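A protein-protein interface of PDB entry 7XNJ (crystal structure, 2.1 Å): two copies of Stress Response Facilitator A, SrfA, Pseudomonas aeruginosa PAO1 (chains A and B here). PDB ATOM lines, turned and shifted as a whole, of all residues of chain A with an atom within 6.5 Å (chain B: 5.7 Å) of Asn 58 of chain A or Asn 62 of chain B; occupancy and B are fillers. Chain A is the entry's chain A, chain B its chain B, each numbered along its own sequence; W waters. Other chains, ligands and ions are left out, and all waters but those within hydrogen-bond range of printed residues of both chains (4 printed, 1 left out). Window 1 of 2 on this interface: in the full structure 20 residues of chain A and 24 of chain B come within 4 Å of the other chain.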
ATOM      1  N   LEU A  26     -30.710 -22.213 -16.982  1.00  0.00           N
ATOM      2  CA  LEU A  26     -29.580 -23.120 -17.176  1.00  0.00           C
ATOM      3  C   LEU A  26     -28.647 -23.117 -15.972  1.00  0.00           C
ATOM      4  O   LEU A  26     -28.114 -24.165 -15.585  1.00  0.00           O
ATOM      5  CB  LEU A  26     -28.797 -22.735 -18.430  1.00  0.00           C
ATOM      6  CG  LEU A  26     -29.499 -22.803 -19.788  1.00  0.00           C
ATOM      7  CD1 LEU A  26     -28.607 -22.202 -20.864  1.00  0.00           C
ATOM      8  CD2 LEU A  26     -29.899 -24.229 -20.143  1.00  0.00           C
ATOM      9  N   ARG A  27     -28.390 -21.935 -15.407  1.00  0.00           N
ATOM     10  CA  ARG A  27     -27.484 -21.828 -14.273  1.00  0.00           C
ATOM     11  C   ARG A  27     -28.072 -22.535 -13.064  1.00  0.00           C
ATOM     12  O   ARG A  27     -27.368 -23.244 -12.338  1.00  0.00           O
ATOM     13  CB  ARG A  27     -27.216 -20.343 -13.987  1.00  0.00           C
ATOM     14  CG  ARG A  27     -26.323 -20.006 -12.782  1.00  0.00           C
ATOM     15  CD  ARG A  27     -24.860 -20.264 -13.072  1.00  0.00           C
ATOM     16  NE  ARG A  27     -24.474 -21.611 -12.667  1.00  0.00           N
ATOM     17  CZ  ARG A  27     -23.573 -22.359 -13.293  1.00  0.00           C
ATOM     18  NH1 ARG A  27     -22.910 -21.907 -14.341  1.00  0.00           N
ATOM     19  NH2 ARG A  27     -23.327 -23.593 -12.846  1.00  0.00           N
ATOM     20  N   ALA A  30     -27.704 -26.387 -13.372  1.00  0.00           N
ATOM     21  CA  ALA A  30     -26.341 -26.879 -13.184  1.00  0.00           C
ATOM     22  C   ALA A  30     -25.954 -26.853 -11.714  1.00  0.00           C
ATOM     23  O   ALA A  30     -25.347 -27.800 -11.200  1.00  0.00           O
ATOM     24  CB  ALA A  30     -25.359 -26.041 -14.005  1.00  0.00           C
ATOM     25  N   ASP A  31     -26.276 -25.759 -11.023  1.00  0.00           N
ATOM     26  CA  ASP A  31     -25.975 -25.686  -9.597  1.00  0.00           C
ATOM     27  C   ASP A  31     -26.756 -26.739  -8.825  1.00  0.00           C
ATOM     28  O   ASP A  31     -26.226 -27.358  -7.896  1.00  0.00           O
ATOM     29  CB  ASP A  31     -26.266 -24.280  -9.078  1.00  0.00           C
ATOM     30  CG  ASP A  31     -25.419 -23.217  -9.767  1.00  0.00           C
ATOM     31  OD1 ASP A  31     -24.372 -23.568 -10.363  1.00  0.00           O
ATOM     32  OD2 ASP A  31     -25.785 -22.027  -9.694  1.00  0.00           O
ATOM     33  N   ALA A  53     -23.011 -35.355 -15.198  1.00  0.00           N
ATOM     34  CA  ALA A  53     -24.173 -34.520 -15.480  1.00  0.00           C
ATOM     35  C   ALA A  53     -23.934 -33.080 -15.047  1.00  0.00           C
ATOM     36  O   ALA A  53     -24.332 -32.135 -15.740  1.00  0.00           O
ATOM     37  CB  ALA A  53     -25.406 -35.086 -14.781  1.00  0.00           C
ATOM     38  N   ALA A  54     -23.294 -32.891 -13.896  1.00  0.00           N
ATOM     39  CA  ALA A  54     -23.030 -31.529 -13.449  1.00  0.00           C
ATOM     40  C   ALA A  54     -22.031 -30.852 -14.367  1.00  0.00           C
ATOM     41  O   ALA A  54     -22.174 -29.666 -14.679  1.00  0.00           O
ATOM     42  CB  ALA A  54     -22.532 -31.533 -12.003  1.00  0.00           C
ATOM     43  N   PHE A  55     -21.018 -31.586 -14.819  1.00  0.00           N
ATOM     44  CA  PHE A  55     -20.075 -31.010 -15.772  1.00  0.00           C
ATOM     45  C   PHE A  55     -20.791 -30.630 -17.064  1.00  0.00           C
ATOM     46  O   PHE A  55     -20.580 -29.540 -17.606  1.00  0.00           O
ATOM     47  CB  PHE A  55     -18.938 -31.997 -16.062  1.00  0.00           C
ATOM     48  CG  PHE A  55     -17.762 -31.885 -15.123  1.00  0.00           C
ATOM     49  CD1 PHE A  55     -17.100 -30.677 -14.950  1.00  0.00           C
ATOM     50  CD2 PHE A  55     -17.314 -32.994 -14.425  1.00  0.00           C
ATOM     51  CE1 PHE A  55     -16.014 -30.576 -14.098  1.00  0.00           C
ATOM     52  CE2 PHE A  55     -16.244 -32.897 -13.565  1.00  0.00           C
ATOM     53  CZ  PHE A  55     -15.597 -31.687 -13.395  1.00  0.00           C
ATOM     54  N   ASP A  56     -21.660 -31.507 -17.555  1.00  0.00           N
ATOM     55  CA  ASP A  56     -22.367 -31.221 -18.793  1.00  0.00           C
ATOM     56  C   ASP A  56     -23.254 -29.988 -18.647  1.00  0.00           C
ATOM     57  O   ASP A  56     -23.239 -29.098 -19.503  1.00  0.00           O
ATOM     58  CB  ASP A  56     -23.190 -32.435 -19.215  1.00  0.00           C
ATOM     59  CG  ASP A  56     -22.327 -33.611 -19.630  1.00  0.00           C
ATOM     60  OD1 ASP A  56     -21.103 -33.429 -19.871  1.00  0.00           O
ATOM     61  OD2 ASP A  56     -22.885 -34.721 -19.751  1.00  0.00           O
ATOM     62  N   LEU A  57     -24.035 -29.912 -17.561  1.00  0.00           N
ATOM     63  CA  LEU A  57     -24.973 -28.797 -17.435  1.00  0.00           C
ATOM     64  C   LEU A  57     -24.251 -27.481 -17.178  1.00  0.00           C
ATOM     65  O   LEU A  57     -24.709 -26.421 -17.625  1.00  0.00           O
ATOM     66  CB  LEU A  57     -25.986 -29.084 -16.321  1.00  0.00           C
ATOM     67  CG  LEU A  57     -26.966 -30.239 -16.557  1.00  0.00           C
ATOM     68  CD1 LEU A  57     -27.485 -30.817 -15.237  1.00  0.00           C
ATOM     69  CD2 LEU A  57     -28.131 -29.778 -17.429  1.00  0.00           C
ATOM     70  N   ASN A  58     -23.128 -27.509 -16.471  1.00  0.00           N
ATOM     71  CA  ASN A  58     -22.404 -26.260 -16.289  1.00  0.00           C
ATOM     72  C   ASN A  58     -21.845 -25.762 -17.608  1.00  0.00           C
ATOM     73  O   ASN A  58     -21.831 -24.549 -17.864  1.00  0.00           O
ATOM     74  CB  ASN A  58     -21.282 -26.419 -15.274  1.00  0.00           C
ATOM     75  CG  ASN A  58     -20.569 -25.101 -15.013  1.00  0.00           C
ATOM     76  OD1 ASN A  58     -21.141 -24.181 -14.412  1.00  0.00           O
ATOM     77  ND2 ASN A  58     -19.338 -24.984 -15.506  1.00  0.00           N
ATOM     78  N   ARG A  59     -21.358 -26.679 -18.452  1.00  0.00           N
ATOM     79  CA  ARG A  59     -20.838 -26.269 -19.751  1.00  0.00           C
ATOM     80  C   ARG A  59     -21.912 -25.556 -20.554  1.00  0.00           C
ATOM     81  O   ARG A  59     -21.653 -24.510 -21.157  1.00  0.00           O
ATOM     82  CB  ARG A  59     -20.300 -27.478 -20.527  1.00  0.00           C
ATOM     83  CG  ARG A  59     -18.913 -27.932 -20.084  1.00  0.00           C
ATOM     84  CD  ARG A  59     -18.180 -28.720 -21.166  1.00  0.00           C
ATOM     85  NE  ARG A  59     -18.972 -29.841 -21.658  1.00  0.00           N
ATOM     86  CZ  ARG A  59     -19.067 -31.014 -21.047  1.00  0.00           C
ATOM     87  NH1 ARG A  59     -18.415 -31.261 -19.921  1.00  0.00           N
ATOM     88  NH2 ARG A  59     -19.821 -31.967 -21.584  1.00  0.00           N
ATOM     89  N   LYS A  60     -23.135 -26.092 -20.540  1.00  0.00           N
ATOM     90  CA  LYS A  60     -24.233 -25.472 -21.277  1.00  0.00           C
ATOM     91  C   LYS A  60     -24.516 -24.066 -20.765  1.00  0.00           C
ATOM     92  O   LYS A  60     -24.669 -23.124 -21.559  1.00  0.00           O
ATOM     93  CB  LYS A  60     -25.489 -26.330 -21.170  1.00  0.00           C
ATOM     94  CG  LYS A  60     -25.618 -27.421 -22.240  1.00  0.00           C
ATOM     95  CD  LYS A  60     -27.006 -28.084 -22.203  1.00  0.00           C
ATOM     96  CE  LYS A  60     -28.099 -27.092 -21.800  1.00  0.00           C
ATOM     97  NZ  LYS A  60     -28.728 -26.405 -22.978  1.00  0.00           N
ATOM     98  N   ALA A  61     -24.585 -23.908 -19.437  1.00  0.00           N
ATOM     99  CA  ALA A  61     -24.893 -22.601 -18.850  1.00  0.00           C
ATOM    100  C   ALA A  61     -23.778 -21.602 -19.107  1.00  0.00           C
ATOM    101  O   ALA A  61     -24.040 -20.445 -19.464  1.00  0.00           O
ATOM    102  CB  ALA A  61     -25.141 -22.727 -17.343  1.00  0.00           C
ATOM    103  N   ASN A  62     -22.528 -22.022 -18.912  1.00  0.00           N
ATOM    104  CA  ASN A  62     -21.411 -21.132 -19.181  1.00  0.00           C
ATOM    105  C   ASN A  62     -21.369 -20.734 -20.653  1.00  0.00           C
ATOM    106  O   ASN A  62     -21.160 -19.558 -20.979  1.00  0.00           O
ATOM    107  CB  ASN A  62     -20.105 -21.796 -18.768  1.00  0.00           C
ATOM    108  CG  ASN A  62     -18.930 -20.860 -18.863  1.00  0.00           C
ATOM    109  OD1 ASN A  62     -18.884 -19.841 -18.179  1.00  0.00           O
ATOM    110  ND2 ASN A  62     -17.967 -21.199 -19.707  1.00  0.00           N
ATOM    111  N   GLN A  63     -21.589 -21.699 -21.556  1.00  0.00           N
ATOM    112  CA  GLN A  63     -21.610 -21.397 -22.986  1.00  0.00           C
ATOM    113  C   GLN A  63     -22.714 -20.400 -23.325  1.00  0.00           C
ATOM    114  O   GLN A  63     -22.557 -19.568 -24.226  1.00  0.00           O
ATOM    115  CB  GLN A  63     -21.788 -22.696 -23.784  1.00  0.00           C
ATOM    116  CG  GLN A  63     -20.495 -23.495 -23.915  1.00  0.00           C
ATOM    117  CD  GLN A  63     -20.712 -24.973 -24.209  1.00  0.00           C
ATOM    118  OE1 GLN A  63     -21.844 -25.439 -24.354  1.00  0.00           O
ATOM    119  NE2 GLN A  63     -19.616 -25.725 -24.271  1.00  0.00           N
ATOM    120  N   GLU A  66     -21.423 -16.945 -22.294  1.00  0.00           N
ATOM    121  CA  GLU A  66     -20.443 -16.433 -23.248  1.00  0.00           C
ATOM    122  C   GLU A  66     -21.080 -16.091 -24.585  1.00  0.00           C
ATOM    123  O   GLU A  66     -20.578 -15.216 -25.300  1.00  0.00           O
ATOM    124  CB  GLU A  66     -19.311 -17.445 -23.451  1.00  0.00           C
ATOM    125  CG  GLU A  66     -18.538 -17.766 -22.195  1.00  0.00           C
ATOM    126  CD  GLU A  66     -17.498 -18.876 -22.403  1.00  0.00           C
ATOM    127  OE1 GLU A  66     -17.651 -19.676 -23.355  1.00  0.00           O
ATOM    128  OE2 GLU A  66     -16.540 -18.967 -21.602  1.00  0.00           O
ATOM    129  N   TYR B  23     -16.300 -17.960  -5.003  1.00  0.00           N
ATOM    130  CA  TYR B  23     -16.899 -18.072  -6.330  1.00  0.00           C
ATOM    131  C   TYR B  23     -17.916 -16.965  -6.573  1.00  0.00           C
ATOM    132  O   TYR B  23     -17.969 -16.386  -7.667  1.00  0.00           O
ATOM    133  CB  TYR B  23     -17.569 -19.434  -6.503  1.00  0.00           C
ATOM    134  CG  TYR B  23     -18.527 -19.429  -7.671  1.00  0.00           C
ATOM    135  CD1 TYR B  23     -18.067 -19.616  -8.977  1.00  0.00           C
ATOM    136  CD2 TYR B  23     -19.881 -19.199  -7.484  1.00  0.00           C
ATOM    137  CE1 TYR B  23     -18.934 -19.580 -10.042  1.00  0.00           C
ATOM    138  CE2 TYR B  23     -20.752 -19.175  -8.541  1.00  0.00           C
ATOM    139  CZ  TYR B  23     -20.278 -19.367  -9.817  1.00  0.00           C
ATOM    140  OH  TYR B  23     -21.158 -19.333 -10.869  1.00  0.00           O
ATOM    141  N   ARG B  27     -18.005 -14.605  -9.667  1.00  0.00           N
ATOM    142  CA  ARG B  27     -19.203 -14.510 -10.510  1.00  0.00           C
ATOM    143  C   ARG B  27     -19.652 -13.058 -10.648  1.00  0.00           C
ATOM    144  O   ARG B  27     -19.878 -12.563 -11.761  1.00  0.00           O
ATOM    145  CB  ARG B  27     -20.329 -15.365  -9.928  1.00  0.00           C
ATOM    146  CG  ARG B  27     -21.598 -15.484 -10.787  1.00  0.00           C
ATOM    147  CD  ARG B  27     -21.331 -16.264 -12.082  1.00  0.00           C
ATOM    148  NE  ARG B  27     -21.057 -15.351 -13.193  1.00  0.00           N
ATOM    149  CZ  ARG B  27     -20.247 -15.599 -14.217  1.00  0.00           C
ATOM    150  NH1 ARG B  27     -19.627 -16.767 -14.351  1.00  0.00           N
ATOM    151  NH2 ARG B  27     -20.060 -14.655 -15.134  1.00  0.00           N
ATOM    152  N   LEU B  57     -12.605 -12.649 -16.924  1.00  0.00           N
ATOM    153  CA  LEU B  57     -13.153 -12.772 -15.575  1.00  0.00           C
ATOM    154  C   LEU B  57     -14.143 -13.925 -15.490  1.00  0.00           C
ATOM    155  O   LEU B  57     -14.119 -14.701 -14.526  1.00  0.00           O
ATOM    156  CB  LEU B  57     -13.812 -11.465 -15.145  1.00  0.00           C
ATOM    157  CG  LEU B  57     -12.861 -10.280 -14.976  1.00  0.00           C
ATOM    158  CD1 LEU B  57     -13.658  -9.009 -14.771  1.00  0.00           C
ATOM    159  CD2 LEU B  57     -11.916 -10.497 -13.806  1.00  0.00           C
ATOM    160  N   ASN B  58     -15.024 -14.056 -16.490  1.00  0.00           N
ATOM    161  CA  ASN B  58     -15.987 -15.160 -16.506  1.00  0.00           C
ATOM    162  C   ASN B  58     -15.292 -16.516 -16.485  1.00  0.00           C
ATOM    163  O   ASN B  58     -15.732 -17.445 -15.788  1.00  0.00           O
ATOM    164  CB  ASN B  58     -16.879 -15.068 -17.738  1.00  0.00           C
ATOM    165  CG  ASN B  58     -17.695 -16.308 -17.933  1.00  0.00           C
ATOM    166  OD1 ASN B  58     -18.619 -16.569 -17.182  1.00  0.00           O
ATOM    167  ND2 ASN B  58     -17.351 -17.095 -18.928  1.00  0.00           N
ATOM    168  N   ARG B  59     -14.218 -16.657 -17.263  1.00  0.00           N
ATOM    169  CA  ARG B  59     -13.458 -17.905 -17.262  1.00  0.00           C
ATOM    170  C   ARG B  59     -12.867 -18.183 -15.885  1.00  0.00           C
ATOM    171  O   ARG B  59     -12.849 -19.332 -15.427  1.00  0.00           O
ATOM    172  CB  ARG B  59     -12.347 -17.852 -18.311  1.00  0.00           C
ATOM    173  CG  ARG B  59     -11.391 -19.022 -18.197  1.00  0.00           C
ATOM    174  CD  ARG B  59      -9.957 -18.685 -18.618  1.00  0.00           C
ATOM    175  NE  ARG B  59      -9.740 -18.767 -20.058  1.00  0.00           N
ATOM    176  CZ  ARG B  59      -9.810 -17.739 -20.894  1.00  0.00           C
ATOM    177  NH1 ARG B  59     -10.118 -16.520 -20.473  1.00  0.00           N
ATOM    178  NH2 ARG B  59      -9.561 -17.936 -22.186  1.00  0.00           N
ATOM    179  N   LYS B  60     -12.355 -17.148 -15.221  1.00  0.00           N
ATOM    180  CA  LYS B  60     -11.836 -17.342 -13.873  1.00  0.00           C
ATOM    181  C   LYS B  60     -12.934 -17.836 -12.945  1.00  0.00           C
ATOM    182  O   LYS B  60     -12.725 -18.774 -12.176  1.00  0.00           O
ATOM    183  CB  LYS B  60     -11.226 -16.044 -13.349  1.00  0.00           C
ATOM    184  CG  LYS B  60     -10.619 -16.143 -11.942  1.00  0.00           C
ATOM    185  CD  LYS B  60      -9.737 -14.929 -11.595  1.00  0.00           C
ATOM    186  CE  LYS B  60      -8.715 -14.641 -12.687  1.00  0.00           C
ATOM    187  NZ  LYS B  60      -7.403 -15.342 -12.445  1.00  0.00           N
ATOM    188  N   ALA B  61     -14.127 -17.237 -13.034  1.00  0.00           N
ATOM    189  CA  ALA B  61     -15.255 -17.689 -12.223  1.00  0.00           C
ATOM    190  C   ALA B  61     -15.716 -19.092 -12.619  1.00  0.00           C
ATOM    191  O   ALA B  61     -16.058 -19.906 -11.753  1.00  0.00           O
ATOM    192  CB  ALA B  61     -16.415 -16.693 -12.344  1.00  0.00           C
ATOM    193  N   ASN B  62     -15.757 -19.389 -13.920  1.00  0.00           N
ATOM    194  CA  ASN B  62     -16.209 -20.708 -14.355  1.00  0.00           C
ATOM    195  C   ASN B  62     -15.233 -21.793 -13.912  1.00  0.00           C
ATOM    196  O   ASN B  62     -15.650 -22.864 -13.452  1.00  0.00           O
ATOM    197  CB  ASN B  62     -16.383 -20.735 -15.878  1.00  0.00           C
ATOM    198  CG  ASN B  62     -16.996 -22.049 -16.373  1.00  0.00           C
ATOM    199  OD1 ASN B  62     -18.018 -22.491 -15.854  1.00  0.00           O
ATOM    200  ND2 ASN B  62     -16.368 -22.675 -17.375  1.00  0.00           N
ATOM    201  N   GLN B  63     -13.930 -21.529 -14.037  1.00  0.00           N
ATOM    202  CA  GLN B  63     -12.938 -22.526 -13.648  1.00  0.00           C
ATOM    203  C   GLN B  63     -12.988 -22.827 -12.151  1.00  0.00           C
ATOM    204  O   GLN B  63     -12.697 -23.951 -11.736  1.00  0.00           O
ATOM    205  CB  GLN B  63     -11.540 -22.043 -14.042  1.00  0.00           C
ATOM    206  CG  GLN B  63     -11.242 -22.143 -15.520  1.00  0.00           C
ATOM    207  CD  GLN B  63      -9.881 -21.583 -15.861  1.00  0.00           C
ATOM    208  OE1 GLN B  63      -9.337 -20.743 -15.133  1.00  0.00           O
ATOM    209  NE2 GLN B  63      -9.313 -22.051 -16.963  1.00  0.00           N
ATOM    210  N   TYR B  64     -13.327 -21.833 -11.334  1.00  0.00           N
ATOM    211  CA  TYR B  64     -13.433 -22.047  -9.887  1.00  0.00           C
ATOM    212  C   TYR B  64     -14.606 -22.956  -9.557  1.00  0.00           C
ATOM    213  O   TYR B  64     -14.491 -23.875  -8.731  1.00  0.00           O
ATOM    214  CB  TYR B  64     -13.584 -20.696  -9.175  1.00  0.00           C
ATOM    215  CG  TYR B  64     -13.067 -20.679  -7.756  1.00  0.00           C
ATOM    216  CD1 TYR B  64     -13.857 -21.115  -6.706  1.00  0.00           C
ATOM    217  CD2 TYR B  64     -11.776 -20.240  -7.466  1.00  0.00           C
ATOM    218  CE1 TYR B  64     -13.387 -21.106  -5.396  1.00  0.00           C
ATOM    219  CE2 TYR B  64     -11.300 -20.234  -6.162  1.00  0.00           C
ATOM    220  CZ  TYR B  64     -12.111 -20.672  -5.134  1.00  0.00           C
ATOM    221  OH  TYR B  64     -11.644 -20.675  -3.841  1.00  0.00           O
ATOM    222  N   TRP B  65     -15.757 -22.689 -10.176  1.00  0.00           N
ATOM    223  CA  TRP B  65     -16.907 -23.575 -10.041  1.00  0.00           C
ATOM    224  C   TRP B  65     -16.531 -24.997 -10.430  1.00  0.00           C
ATOM    225  O   TRP B  65     -16.909 -25.952  -9.751  1.00  0.00           O
ATOM    226  CB  TRP B  65     -18.049 -23.067 -10.922  1.00  0.00           C
ATOM    227  CG  TRP B  65     -19.410 -23.679 -10.686  1.00  0.00           C
ATOM    228  CD1 TRP B  65     -20.461 -23.118 -10.006  1.00  0.00           C
ATOM    229  CD2 TRP B  65     -19.886 -24.944 -11.188  1.00  0.00           C
ATOM    230  NE1 TRP B  65     -21.551 -23.967 -10.036  1.00  0.00           N
ATOM    231  CE2 TRP B  65     -21.217 -25.097 -10.742  1.00  0.00           C
ATOM    232  CE3 TRP B  65     -19.306 -25.968 -11.943  1.00  0.00           C
ATOM    233  CZ2 TRP B  65     -21.976 -26.227 -11.040  1.00  0.00           C
ATOM    234  CZ3 TRP B  65     -20.062 -27.102 -12.232  1.00  0.00           C
ATOM    235  CH2 TRP B  65     -21.385 -27.219 -11.784  1.00  0.00           C
ATOM    236  N   GLU B  66     -15.792 -25.151 -11.531  1.00  0.00           N
ATOM    237  CA  GLU B  66     -15.439 -26.484 -12.002  1.00  0.00           C
ATOM    238  C   GLU B  66     -14.439 -27.171 -11.081  1.00  0.00           C
ATOM    239  O   GLU B  66     -14.438 -28.402 -10.986  1.00  0.00           O
ATOM    240  CB  GLU B  66     -14.865 -26.417 -13.417  1.00  0.00           C
ATOM    241  CG  GLU B  66     -15.853 -26.038 -14.479  1.00  0.00           C
ATOM    242  CD  GLU B  66     -15.174 -25.885 -15.824  1.00  0.00           C
ATOM    243  OE1 GLU B  66     -13.957 -25.571 -15.856  1.00  0.00           O
ATOM    244  OE2 GLU B  66     -15.854 -26.073 -16.843  1.00  0.00           O
ATOM    245  N   GLN B  67     -13.546 -26.407 -10.445  1.00  0.00           N
ATOM    246  CA  GLN B  67     -12.617 -26.999  -9.490  1.00  0.00           C
ATOM    247  C   GLN B  67     -13.359 -27.448  -8.232  1.00  0.00           C
ATOM    248  O   GLN B  67     -13.081 -28.519  -7.682  1.00  0.00           O
ATOM    249  CB  GLN B  67     -11.526 -25.984  -9.155  1.00  0.00           C
ATOM    250  CG  GLN B  67     -10.488 -26.461  -8.154  1.00  0.00           C
ATOM    251  CD  GLN B  67      -9.756 -27.672  -8.658  1.00  0.00           C
ATOM    252  OE1 GLN B  67      -9.125 -27.630  -9.711  1.00  0.00           O
ATOM    253  NE2 GLN B  67      -9.880 -28.779  -7.938  1.00  0.00           N
HETATM  254  O   HOH W   1     -18.267 -27.624 -16.637  1.00  0.00           O
HETATM  255  O   HOH W   2     -19.484 -21.784 -13.904  1.00  0.00           O
HETATM  256  O   HOH W   3     -15.338 -16.989 -20.487  1.00  0.00           O
HETATM  257  O   HOH W   4     -23.722 -20.539  -9.117  1.00  0.00           O
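Water W2 lies within hydrogen-bond range of the side-chain amide oxygen (OD1) of Asn 62 of chain B, the side-chain amide oxygen (OD1) of Asn 58 of chain A and the guanidinium group (NH1) of Arg 27 of chain A. Water W3 lies within hydrogen-bond range of ND2 of Asn 58 of chain B, OE2 of Glu 66 of chain A and N of Arg 59 of chain B. Water W4 lies within hydrogen-bond range of OD2 of Asp 31 of chain A (2.6 Å) and OH of Tyr 23 of chain B (3.3 Å). Water W1 lies within hydrogen-bond range of the side-chain carboxylate (OE2) of Glu 66 of chain B, the side-chain amide nitrogen (ND2) of Asn 58 of chain A and the backbone carbonyl oxygen (O) of Phe 55 of chain A.
Ala 30 of chain A touches Trp 65 of chain B. Trp 65 of chain B touches Ala 54 of chain A. Trp 65 of chain B touches Asn 58 of chain A. ND2 of Asn 58 of chain A touches CG of Glu 66 of chain B (3.8 Å).
Asn 58 of chain A touches Asn 62 of chain B, and with the chains exchanged Asn 62 of chain A touches Asn 58 of chain B. Asn 58 of chain A touches Glu 66 of chain B, and with the chains exchanged Glu 66 of chain A touches Asn 58 of chain B. Asn 62 of chain B touches its own counterpart, Asn 62 of chain A.
The side-chain carboxylate of Asp 31 of chain A is in hydrogen-bond range of the indole nitrogen of Trp 65 of chain B. The side-chain amide oxygen (OD1) of Asn 62 of chain B is in hydrogen-bond range of the side-chain amide nitrogen (ND2) of Asn 58 of chain A (2.8 Å). The side-chain amide oxygen of Asn 62 of chain A lies within hydrogen-bond range of the side-chain amide nitrogen of Asn 58 of chain B. The side-chain amide nitrogen of Asn 62 of chain A sits close to the side-chain amide nitrogen of Asn 62 of chain B (3.2 Å). OE2 of Glu 66 of chain A sits at hydrogen-bond distance from ND2 of Asn 58 of chain B, at 3.4 Å. The guanidinium group of Arg 27 of chain A lies close to the indole nitrogen of Trp 65 of chain B (3.3 Å).
Among the printed residues, no Asp or Glu carboxylate lies within 4 Å of a Lys or Arg side-chain nitrogen of the other chain.
The guanidinium group (NH2) of Arg 27 of chain A lies within salt-bridge range of the side-chain carboxylate (OD1) of Asp 31 of chain A (2.7 Å). The guanidinium group of Arg 27 of chain A is in hydrogen-bond range of the side-chain amide oxygen of Asn 58 of chain A (2.8 Å). ND2 of Asn 62 of chain A lies within hydrogen-bond range of OE2 of Glu 66 of chain A. The side-chain amide oxygen (OD1) of Asn 58 of chain B sits at hydrogen-bond distance from the guanidinium group (NH1) of Arg 27 of chain B. The side-chain amide nitrogen (ND2) of Asn 62 of chain B sits at hydrogen-bond distance from the side-chain carboxylate (OE2) of Glu 66 of chain B.
Of the printed residues of chain B, Ala 30 of chain A touches Trp 65 (3.7 Å). Of the printed residues of chain B, Ala 54 of chain A touches Trp 65. Asn 58 of chain A touches just these residues of chain B: Asn 62 (2.8 Å), Trp 65 (3.3 Å) and Glu 66 (3.8 Å). Printed residues of chain B within 4 Å of Glu 66 of chain A: Asn 58. Asn 62 of chain B touches just these residues of chain A: Asn 58 (2.8 Å) and Asn 62 (3.2 Å). Of the printed residues of chain A, Glu 66 of chain B touches Asn 58 (3.8 Å). The nearest printed residue of chain B that does not touch Asn 58 of chain A is Tyr 23 of chain B (6.0 Å).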
